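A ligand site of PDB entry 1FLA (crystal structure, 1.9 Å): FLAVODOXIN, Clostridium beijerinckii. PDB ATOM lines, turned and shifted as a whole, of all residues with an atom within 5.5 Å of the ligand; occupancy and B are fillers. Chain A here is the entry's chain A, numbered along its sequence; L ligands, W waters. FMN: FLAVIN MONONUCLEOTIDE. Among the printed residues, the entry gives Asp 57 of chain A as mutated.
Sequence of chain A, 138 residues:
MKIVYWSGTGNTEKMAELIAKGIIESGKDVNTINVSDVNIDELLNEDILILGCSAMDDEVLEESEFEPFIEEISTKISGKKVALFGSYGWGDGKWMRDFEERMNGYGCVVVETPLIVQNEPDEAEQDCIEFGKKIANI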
ATOM      1  N   TRP A   6     -37.854 -29.368 -17.281  1.00  0.00           N
ATOM      2  CA  TRP A   6     -37.466 -30.132 -16.106  1.00  0.00           C
ATOM      3  C   TRP A   6     -36.372 -29.289 -15.470  1.00  0.00           C
ATOM      4  O   TRP A   6     -35.516 -28.754 -16.188  1.00  0.00           O
ATOM      5  CB  TRP A   6     -36.891 -31.513 -16.445  1.00  0.00           C
ATOM      6  CG  TRP A   6     -36.632 -32.286 -15.159  1.00  0.00           C
ATOM      7  CD1 TRP A   6     -37.560 -32.962 -14.413  1.00  0.00           C
ATOM      8  CD2 TRP A   6     -35.399 -32.328 -14.409  1.00  0.00           C
ATOM      9  NE1 TRP A   6     -36.987 -33.403 -13.236  1.00  0.00           N
ATOM     10  CE2 TRP A   6     -35.669 -33.022 -13.201  1.00  0.00           C
ATOM     11  CE3 TRP A   6     -34.101 -31.833 -14.631  1.00  0.00           C
ATOM     12  CZ2 TRP A   6     -34.681 -33.241 -12.222  1.00  0.00           C
ATOM     13  CZ3 TRP A   6     -33.117 -32.063 -13.642  1.00  0.00           C
ATOM     14  CH2 TRP A   6     -33.421 -32.758 -12.459  1.00  0.00           C
ATOM     15  N   SER A   7     -36.396 -29.145 -14.151  1.00  0.00           N
ATOM     16  CA  SER A   7     -35.360 -28.411 -13.440  1.00  0.00           C
ATOM     17  C   SER A   7     -35.097 -29.063 -12.090  1.00  0.00           C
ATOM     18  O   SER A   7     -36.024 -29.277 -11.320  1.00  0.00           O
ATOM     19  CB  SER A   7     -35.768 -26.942 -13.262  1.00  0.00           C
ATOM     20  OG  SER A   7     -34.724 -26.180 -12.655  1.00  0.00           O
ATOM     21  N   GLY A   8     -33.818 -29.326 -11.800  1.00  0.00           N
ATOM     22  CA  GLY A   8     -33.446 -29.958 -10.537  1.00  0.00           C
ATOM     23  C   GLY A   8     -33.199 -29.014  -9.386  1.00  0.00           C
ATOM     24  O   GLY A   8     -33.484 -29.359  -8.245  1.00  0.00           O
ATOM     25  N   THR A   9     -32.616 -27.852  -9.664  1.00  0.00           N
ATOM     26  CA  THR A   9     -32.330 -26.870  -8.616  1.00  0.00           C
ATOM     27  C   THR A   9     -33.023 -25.517  -8.881  1.00  0.00           C
ATOM     28  O   THR A   9     -32.963 -24.614  -8.048  1.00  0.00           O
ATOM     29  CB  THR A   9     -30.808 -26.651  -8.403  1.00  0.00           C
ATOM     30  OG1 THR A   9     -30.271 -25.880  -9.475  1.00  0.00           O
ATOM     31  CG2 THR A   9     -30.082 -27.979  -8.362  1.00  0.00           C
ATOM     32  N   GLY A  10     -33.658 -25.386 -10.044  1.00  0.00           N
ATOM     33  CA  GLY A  10     -34.372 -24.165 -10.357  1.00  0.00           C
ATOM     34  C   GLY A  10     -33.732 -23.260 -11.370  1.00  0.00           C
ATOM     35  O   GLY A  10     -34.291 -22.207 -11.684  1.00  0.00           O
ATOM     36  N   ASN A  11     -32.602 -23.657 -11.931  1.00  0.00           N
ATOM     37  CA  ASN A  11     -31.927 -22.812 -12.919  1.00  0.00           C
ATOM     38  C   ASN A  11     -32.672 -22.778 -14.262  1.00  0.00           C
ATOM     39  O   ASN A  11     -32.922 -21.695 -14.820  1.00  0.00           O
ATOM     40  CB  ASN A  11     -30.464 -23.244 -13.091  1.00  0.00           C
ATOM     41  CG  ASN A  11     -29.621 -22.989 -11.855  1.00  0.00           C
ATOM     42  OD1 ASN A  11     -28.576 -23.598 -11.661  1.00  0.00           O
ATOM     43  ND2 ASN A  11     -30.081 -22.084 -11.010  1.00  0.00           N
ATOM     44  N   THR A  12     -33.065 -23.947 -14.747  1.00  0.00           N
ATOM     45  CA  THR A  12     -33.834 -24.061 -15.989  1.00  0.00           C
ATOM     46  C   THR A  12     -35.269 -23.517 -15.786  1.00  0.00           C
ATOM     47  O   THR A  12     -35.869 -22.970 -16.707  1.00  0.00           O
ATOM     48  CB  THR A  12     -33.874 -25.524 -16.480  1.00  0.00           C
ATOM     49  OG1 THR A  12     -32.532 -25.969 -16.700  1.00  0.00           O
ATOM     50  CG2 THR A  12     -34.627 -25.630 -17.792  1.00  0.00           C
ATOM     51  N   GLU A  13     -35.783 -23.654 -14.567  1.00  0.00           N
ATOM     52  CA  GLU A  13     -37.106 -23.156 -14.234  1.00  0.00           C
ATOM     53  C   GLU A  13     -37.101 -21.628 -14.348  1.00  0.00           C
ATOM     54  O   GLU A  13     -38.052 -21.035 -14.838  1.00  0.00           O
ATOM     55  CB  GLU A  13     -37.499 -23.566 -12.812  1.00  0.00           C
ATOM     56  CG  GLU A  13     -38.893 -23.057 -12.410  1.00  0.00           C
ATOM     57  CD  GLU A  13     -39.309 -23.417 -10.987  1.00  0.00           C
ATOM     58  OE1 GLU A  13     -38.465 -23.551 -10.086  1.00  0.00           O
ATOM     59  OE2 GLU A  13     -40.531 -23.510 -10.764  1.00  0.00           O
ATOM     60  N   SER A  54     -31.977 -29.167 -18.053  1.00  0.00           N
ATOM     61  CA  SER A  54     -30.567 -28.987 -17.743  1.00  0.00           C
ATOM     62  C   SER A  54     -29.759 -30.234 -18.111  1.00  0.00           C
ATOM     63  O   SER A  54     -30.329 -31.319 -18.313  1.00  0.00           O
ATOM     64  CB  SER A  54     -30.406 -28.716 -16.246  1.00  0.00           C
ATOM     65  OG  SER A  54     -31.088 -29.708 -15.505  1.00  0.00           O
ATOM     66  N   ALA A  55     -28.442 -30.067 -18.224  1.00  0.00           N
ATOM     67  CA  ALA A  55     -27.540 -31.181 -18.537  1.00  0.00           C
ATOM     68  C   ALA A  55     -27.498 -32.069 -17.291  1.00  0.00           C
ATOM     69  O   ALA A  55     -27.306 -31.577 -16.163  1.00  0.00           O
ATOM     70  CB  ALA A  55     -26.158 -30.648 -18.868  1.00  0.00           C
ATOM     71  N   MET A  56     -27.729 -33.369 -17.495  1.00  0.00           N
ATOM     72  CA  MET A  56     -27.736 -34.331 -16.394  1.00  0.00           C
ATOM     73  C   MET A  56     -26.791 -35.512 -16.593  1.00  0.00           C
ATOM     74  O   MET A  56     -26.351 -35.804 -17.704  1.00  0.00           O
ATOM     75  CB  MET A  56     -29.169 -34.837 -16.128  1.00  0.00           C
ATOM     76  CG  MET A  56     -30.019 -33.908 -15.275  1.00  0.00           C
ATOM     77  SD  MET A  56     -29.387 -33.734 -13.572  1.00  0.00           S
ATOM     78  CE  MET A  56     -29.313 -35.453 -13.155  1.00  0.00           C
ATOM     79  N   ASP A  57     -26.474 -36.169 -15.491  1.00  0.00           N
ATOM     80  CA  ASP A  57     -25.572 -37.315 -15.471  1.00  0.00           C
ATOM     81  C   ASP A  57     -24.321 -37.016 -16.277  1.00  0.00           C
ATOM     82  O   ASP A  57     -23.540 -36.155 -15.914  1.00  0.00           O
ATOM     83  CB  ASP A  57     -26.306 -38.570 -15.958  1.00  0.00           C
ATOM     84  CG  ASP A  57     -27.476 -38.915 -15.055  1.00  0.00           C
ATOM     85  OD1 ASP A  57     -27.393 -38.632 -13.825  1.00  0.00           O
ATOM     86  OD2 ASP A  57     -28.494 -39.443 -15.549  1.00  0.00           O
ATOM     87  N   ASP A  58     -24.106 -37.741 -17.360  1.00  0.00           N
ATOM     88  CA  ASP A  58     -22.959 -37.454 -18.174  1.00  0.00           C
ATOM     89  C   ASP A  58     -23.429 -36.926 -19.538  1.00  0.00           C
ATOM     90  O   ASP A  58     -23.562 -37.673 -20.498  1.00  0.00           O
ATOM     91  CB  ASP A  58     -22.073 -38.675 -18.331  1.00  0.00           C
ATOM     92  CG  ASP A  58     -20.771 -38.352 -19.021  1.00  0.00           C
ATOM     93  OD1 ASP A  58     -20.320 -37.182 -18.932  1.00  0.00           O
ATOM     94  OD2 ASP A  58     -20.217 -39.271 -19.667  1.00  0.00           O
ATOM     95  N   GLU A  59     -23.709 -35.630 -19.565  1.00  0.00           N
ATOM     96  CA  GLU A  59     -24.165 -34.918 -20.755  1.00  0.00           C
ATOM     97  C   GLU A  59     -25.371 -35.524 -21.450  1.00  0.00           C
ATOM     98  O   GLU A  59     -25.352 -35.715 -22.673  1.00  0.00           O
ATOM     99  CB  GLU A  59     -23.021 -34.705 -21.752  1.00  0.00           C
ATOM    100  CG  GLU A  59     -21.852 -33.833 -21.227  1.00  0.00           C
ATOM    101  CD  GLU A  59     -22.163 -32.335 -21.131  1.00  0.00           C
ATOM    102  OE1 GLU A  59     -23.182 -31.853 -21.634  1.00  0.00           O
ATOM    103  OE2 GLU A  59     -21.340 -31.627 -20.534  1.00  0.00           O
ATOM    104  N   VAL A  60     -26.425 -35.791 -20.685  1.00  0.00           N
ATOM    105  CA  VAL A  60     -27.673 -36.345 -21.247  1.00  0.00           C
ATOM    106  C   VAL A  60     -28.877 -35.608 -20.658  1.00  0.00           C
ATOM    107  O   VAL A  60     -28.736 -34.793 -19.749  1.00  0.00           O
ATOM    108  CB  VAL A  60     -27.833 -37.871 -20.958  1.00  0.00           C
ATOM    109  CG1 VAL A  60     -26.737 -38.672 -21.653  1.00  0.00           C
ATOM    110  CG2 VAL A  60     -27.837 -38.142 -19.441  1.00  0.00           C
ATOM    111  N   SER A  87     -30.078 -25.033 -18.735  1.00  0.00           N
ATOM    112  CA  SER A  87     -28.923 -24.625 -17.949  1.00  0.00           C
ATOM    113  C   SER A  87     -27.944 -25.808 -17.877  1.00  0.00           C
ATOM    114  O   SER A  87     -28.329 -26.979 -18.025  1.00  0.00           O
ATOM    115  CB  SER A  87     -29.377 -24.246 -16.534  1.00  0.00           C
ATOM    116  OG  SER A  87     -28.277 -23.739 -15.782  1.00  0.00           O
ATOM    117  N   TYR A  88     -26.671 -25.503 -17.665  1.00  0.00           N
ATOM    118  CA  TYR A  88     -25.655 -26.535 -17.560  1.00  0.00           C
ATOM    119  C   TYR A  88     -24.602 -26.053 -16.547  1.00  0.00           C
ATOM    120  O   TYR A  88     -24.648 -24.891 -16.094  1.00  0.00           O
ATOM    121  CB  TYR A  88     -25.046 -26.861 -18.937  1.00  0.00           C
ATOM    122  CG  TYR A  88     -24.284 -25.715 -19.564  1.00  0.00           C
ATOM    123  CD1 TYR A  88     -24.963 -24.671 -20.204  1.00  0.00           C
ATOM    124  CD2 TYR A  88     -22.897 -25.672 -19.518  1.00  0.00           C
ATOM    125  CE1 TYR A  88     -24.277 -23.615 -20.794  1.00  0.00           C
ATOM    126  CE2 TYR A  88     -22.192 -24.616 -20.101  1.00  0.00           C
ATOM    127  CZ  TYR A  88     -22.893 -23.592 -20.738  1.00  0.00           C
ATOM    128  OH  TYR A  88     -22.199 -22.577 -21.346  1.00  0.00           O
ATOM    129  N   GLY A  89     -23.694 -26.940 -16.176  1.00  0.00           N
ATOM    130  CA  GLY A  89     -22.725 -26.578 -15.160  1.00  0.00           C
ATOM    131  C   GLY A  89     -21.273 -26.525 -15.529  1.00  0.00           C
ATOM    132  O   GLY A  89     -20.650 -25.481 -15.350  1.00  0.00           O
ATOM    133  N   TRP A  90     -20.728 -27.611 -16.058  1.00  0.00           N
ATOM    134  CA  TRP A  90     -19.302 -27.637 -16.381  1.00  0.00           C
ATOM    135  C   TRP A  90     -18.883 -27.948 -17.822  1.00  0.00           C
ATOM    136  O   TRP A  90     -17.745 -27.700 -18.199  1.00  0.00           O
ATOM    137  CB  TRP A  90     -18.581 -28.582 -15.416  1.00  0.00           C
ATOM    138  CG  TRP A  90     -19.222 -29.939 -15.307  1.00  0.00           C
ATOM    139  CD1 TRP A  90     -19.060 -30.980 -16.179  1.00  0.00           C
ATOM    140  CD2 TRP A  90     -20.138 -30.398 -14.303  1.00  0.00           C
ATOM    141  NE1 TRP A  90     -19.831 -32.042 -15.783  1.00  0.00           N
ATOM    142  CE2 TRP A  90     -20.502 -31.713 -14.633  1.00  0.00           C
ATOM    143  CE3 TRP A  90     -20.690 -29.817 -13.144  1.00  0.00           C
ATOM    144  CZ2 TRP A  90     -21.395 -32.467 -13.861  1.00  0.00           C
ATOM    145  CZ3 TRP A  90     -21.580 -30.571 -12.382  1.00  0.00           C
ATOM    146  CH2 TRP A  90     -21.920 -31.887 -12.746  1.00  0.00           C
ATOM    147  N   GLY A  91     -19.807 -28.502 -18.612  1.00  0.00           N
ATOM    148  CA  GLY A  91     -19.493 -28.843 -19.975  1.00  0.00           C
ATOM    149  C   GLY A  91     -19.601 -27.637 -20.878  1.00  0.00           C
ATOM    150  O   GLY A  91     -19.564 -26.494 -20.414  1.00  0.00           O
ATOM    151  N   ASP A  92     -19.700 -27.882 -22.179  1.00  0.00           N
ATOM    152  CA  ASP A  92     -19.835 -26.808 -23.143  1.00  0.00           C
ATOM    153  C   ASP A  92     -21.057 -27.000 -24.045  1.00  0.00           C
ATOM    154  O   ASP A  92     -21.043 -26.599 -25.208  1.00  0.00           O
ATOM    155  CB  ASP A  92     -18.539 -26.639 -23.972  1.00  0.00           C
ATOM    156  CG  ASP A  92     -18.144 -27.913 -24.738  1.00  0.00           C
ATOM    157  OD1 ASP A  92     -19.012 -28.774 -25.017  1.00  0.00           O
ATOM    158  OD2 ASP A  92     -16.940 -28.023 -25.093  1.00  0.00           O
ATOM    159  N   GLN A 118     -25.099 -20.995 -18.386  1.00  0.00           N
ATOM    160  CA  GLN A 118     -24.386 -21.688 -17.332  1.00  0.00           C
ATOM    161  C   GLN A 118     -24.879 -21.300 -15.954  1.00  0.00           C
ATOM    162  O   GLN A 118     -24.950 -20.102 -15.629  1.00  0.00           O
ATOM    163  CB  GLN A 118     -22.891 -21.417 -17.441  1.00  0.00           C
ATOM    164  CG  GLN A 118     -22.045 -22.261 -16.526  1.00  0.00           C
ATOM    165  CD  GLN A 118     -20.573 -21.993 -16.740  1.00  0.00           C
ATOM    166  OE1 GLN A 118     -20.177 -20.886 -17.112  1.00  0.00           O
ATOM    167  NE2 GLN A 118     -19.751 -23.015 -16.496  1.00  0.00           N
ATOM    168  N   ASN A 119     -25.251 -22.296 -15.156  1.00  0.00           N
ATOM    169  CA  ASN A 119     -25.743 -22.078 -13.795  1.00  0.00           C
ATOM    170  C   ASN A 119     -26.985 -21.178 -13.836  1.00  0.00           C
ATOM    171  O   ASN A 119     -27.743 -21.225 -14.807  1.00  0.00           O
ATOM    172  CB  ASN A 119     -24.613 -21.508 -12.904  1.00  0.00           C
ATOM    173  CG  ASN A 119     -23.304 -22.301 -13.044  1.00  0.00           C
ATOM    174  OD1 ASN A 119     -23.223 -23.481 -12.678  1.00  0.00           O
ATOM    175  ND2 ASN A 119     -22.297 -21.661 -13.630  1.00  0.00           N
ATOM    176  N   GLU A 120     -27.227 -20.365 -12.798  1.00  0.00           N
ATOM    177  CA  GLU A 120     -28.411 -19.503 -12.793  1.00  0.00           C
ATOM    178  C   GLU A 120     -28.266 -18.387 -13.842  1.00  0.00           C
ATOM    179  O   GLU A 120     -27.169 -17.885 -14.047  1.00  0.00           O
ATOM    180  CB  GLU A 120     -28.626 -18.910 -11.396  1.00  0.00           C
ATOM    181  CG  GLU A 120     -30.009 -18.266 -11.196  1.00  0.00           C
ATOM    182  CD  GLU A 120     -30.114 -17.415  -9.934  1.00  0.00           C
ATOM    183  OE1 GLU A 120     -29.059 -16.975  -9.391  1.00  0.00           O
ATOM    184  OE2 GLU A 120     -31.252 -17.171  -9.481  1.00  0.00           O
HETATM  185  N1  FMN L   1     -23.603 -29.900 -16.189  1.00  0.00           N
HETATM  186  C2  FMN L   1     -22.863 -30.028 -17.337  1.00  0.00           C
HETATM  187  O2  FMN L   1     -22.407 -29.065 -17.908  1.00  0.00           O
HETATM  188  N3  FMN L   1     -22.634 -31.338 -17.866  1.00  0.00           N
HETATM  189  C4  FMN L   1     -23.067 -32.521 -17.282  1.00  0.00           C
HETATM  190  O4  FMN L   1     -22.812 -33.630 -17.783  1.00  0.00           O
HETATM  191  C4A FMN L   1     -23.865 -32.341 -16.019  1.00  0.00           C
HETATM  192  N5  FMN L   1     -24.268 -33.400 -15.328  1.00  0.00           N
HETATM  193  C5A FMN L   1     -24.822 -33.197 -14.110  1.00  0.00           C
HETATM  194  C6  FMN L   1     -25.101 -34.321 -13.295  1.00  0.00           C
HETATM  195  C7  FMN L   1     -25.720 -34.180 -12.101  1.00  0.00           C
HETATM  196  C7M FMN L   1     -26.006 -35.363 -11.234  1.00  0.00           C
HETATM  197  C8  FMN L   1     -26.084 -32.893 -11.634  1.00  0.00           C
HETATM  198  C8M FMN L   1     -26.823 -32.721 -10.327  1.00  0.00           C
HETATM  199  C9  FMN L   1     -25.764 -31.777 -12.390  1.00  0.00           C
HETATM  200  C9A FMN L   1     -25.159 -31.909 -13.633  1.00  0.00           C
HETATM  201  N10 FMN L   1     -24.738 -30.831 -14.370  1.00  0.00           N
HETATM  202  C10 FMN L   1     -24.093 -30.962 -15.576  1.00  0.00           C
HETATM  203  C1' FMN L   1     -24.922 -29.509 -13.792  1.00  0.00           C
HETATM  204  C2' FMN L   1     -26.319 -28.927 -14.047  1.00  0.00           C
HETATM  205  O2' FMN L   1     -26.657 -29.037 -15.433  1.00  0.00           O
HETATM  206  C3' FMN L   1     -26.314 -27.457 -13.688  1.00  0.00           C
HETATM  207  O3' FMN L   1     -26.104 -27.317 -12.277  1.00  0.00           O
HETATM  208  C4' FMN L   1     -27.599 -26.746 -14.074  1.00  0.00           C
HETATM  209  O4' FMN L   1     -27.499 -25.384 -13.675  1.00  0.00           O
HETATM  210  C5' FMN L   1     -28.790 -27.366 -13.345  1.00  0.00           C
HETATM  211  O5' FMN L   1     -29.968 -26.653 -13.701  1.00  0.00           O
HETATM  212  P   FMN L   1     -31.338 -27.037 -13.025  1.00  0.00           P
HETATM  213  O1P FMN L   1     -31.408 -28.475 -12.863  1.00  0.00           O
HETATM  214  O2P FMN L   1     -32.329 -26.416 -13.939  1.00  0.00           O
HETATM  215  O3P FMN L   1     -31.493 -26.434 -11.648  1.00  0.00           O
HETATM  216  O   HOH W   1     -27.735 -29.010 -10.572  1.00  0.00           O
HETATM  217  O   HOH W   2     -22.810 -29.064 -21.146  1.00  0.00           O
HETATM  218  O   HOH W   3     -25.205 -24.959 -11.350  1.00  0.00           O
HETATM  219  O   HOH W   4     -20.419 -34.535 -17.445  1.00  0.00           O
HETATM  220  O   HOH W   5     -29.939 -30.266 -11.418  1.00  0.00           O
HETATM  221  O   HOH W   6     -29.046 -31.226 -14.282  1.00  0.00           O
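N of Ser 87 sits at hydrogen-bond distance from OG1 of Thr 12 (3.3 Å). The backbone carbonyl oxygen (O) of Ser 87 sits at hydrogen-bond distance from the backbone NH (N) of Ala 55 (3.1 Å). OG of Ser 7 sits at hydrogen-bond distance from N of Gly 10, 2.9 Å away. The side-chain hydroxyl (OG) of Ser 7 is in hydrogen-bond range of the backbone NH (N) of Asn 11, at 3.4 Å. The backbone NH (N) of Glu 13 lies within hydrogen-bond range of the side-chain hydroxyl (OG) of Ser 7. The side-chain hydroxyl (OG) of Ser 87 sits at hydrogen-bond distance from the backbone carbonyl oxygen (O) of Asn 119 (2.7 Å). The backbone carbonyl oxygen (O) of Gly 89 lies within hydrogen-bond range of the side-chain amide nitrogen (NE2) of Gln 118 (2.9 Å). N of Asn 119 is in hydrogen-bond range of O of Tyr 88.
N of Thr 9 sits at hydrogen-bond distance from O3P of the ligand (2.7 Å). The side-chain hydroxyl of Thr 9 is in hydrogen-bond range of an oxygen (O3P) of the ligand, 2.6 Å away. The backbone NH of Thr 12 is in hydrogen-bond range of an oxygen (O2P) of the ligand (2.7 Å). O2P of the ligand is in hydrogen-bond range of OG1 of Thr 12 (2.8 Å). The backbone NH of Ala 55 lies within hydrogen-bond range of an oxygen (O2') of the ligand (3.5 Å). An oxygen (O2') of the ligand sits at hydrogen-bond distance from the backbone carbonyl oxygen (O) of Ala 55 (2.7 Å). The side-chain hydroxyl (OG) of Ser 7 is in hydrogen-bond range of an oxygen (O2P) of the ligand. An oxygen (O2) of the ligand is in hydrogen-bond range of the backbone NH of Gly 91. N of Gly 8 sits at hydrogen-bond distance from O1P of the ligand (2.8 Å). O4' of the ligand lies within hydrogen-bond range of OG of Ser 87, at 2.8 Å. The backbone NH (N) of Glu 59 sits at hydrogen-bond distance from an oxygen (O4) of the ligand. The side-chain carboxylate (OE2) of Glu 59 sits at hydrogen-bond distance from a nitrogen (N3) of the ligand (3.0 Å). The backbone NH of Trp 90 sits at hydrogen-bond distance from an oxygen (O2) of the ligand (2.9 Å). An oxygen (O3P) of the ligand sits at hydrogen-bond distance from the backbone NH of Gly 10, 2.9 Å away. N of Asn 11 lies within hydrogen-bond range of O3P of the ligand, 3.0 Å away. The side-chain amide oxygen of Asn 11 sits at hydrogen-bond distance from an oxygen (O4') of the ligand (2.9 Å). O1P of the ligand lies within hydrogen-bond range of OG of Ser 54 (2.9 Å). N of Gly 89 lies within hydrogen-bond range of N1 of the ligand, 3.0 Å away.
Water W4 lies within hydrogen-bond range of O4 of the ligand, OD1 of Asp 58 and NE1 of Trp 90. Water W3 bridges O3' of the ligand and OD1 of Asn 119. Water W2 lies within hydrogen-bond range of the side-chain carboxylate of Glu 59, an oxygen (O2) of the ligand and the backbone NH of Asp 92. Water W6 lies within hydrogen-bond range of the backbone carbonyl oxygen (O) of Ala 55 (2.6 Å), the side-chain sulfur (SD) of Met 56 (2.6 Å), the side-chain hydroxyl (OG) of Ser 54 (2.8 Å) and an oxygen (O2') of the ligand (3.4 Å).
The backbone carbonyl oxygen (O) of Asp 57 lies close to a nitrogen (N5) of the ligand. Merely in contact with the ligand: Tyr 88 (3.4 Å), Met 56 (3.5 Å), Asn 119 (3.7 Å) and Asp 58 (3.8 Å). Hydrophobic or aromatic side chains within 4 Å of the ligand: Ala 55, Met 56, Tyr 88 and Trp 90. Within 4 Å of the ligand: Ser 7, Gly 8, Thr 9, Gly 10, Asn 11, Thr 12, Ser 54, Ala 55, Met 56, Asp 57, Asp 58, Glu 59, Ser 87, Tyr 88, Gly 89, Trp 90, Gly 91 and Asn 119. Along chain A the residues within 4 Å of the ligand span positions 7 to 119. The nearest printed residue that does not touch the ligand is Trp 6 (4.05 Å).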
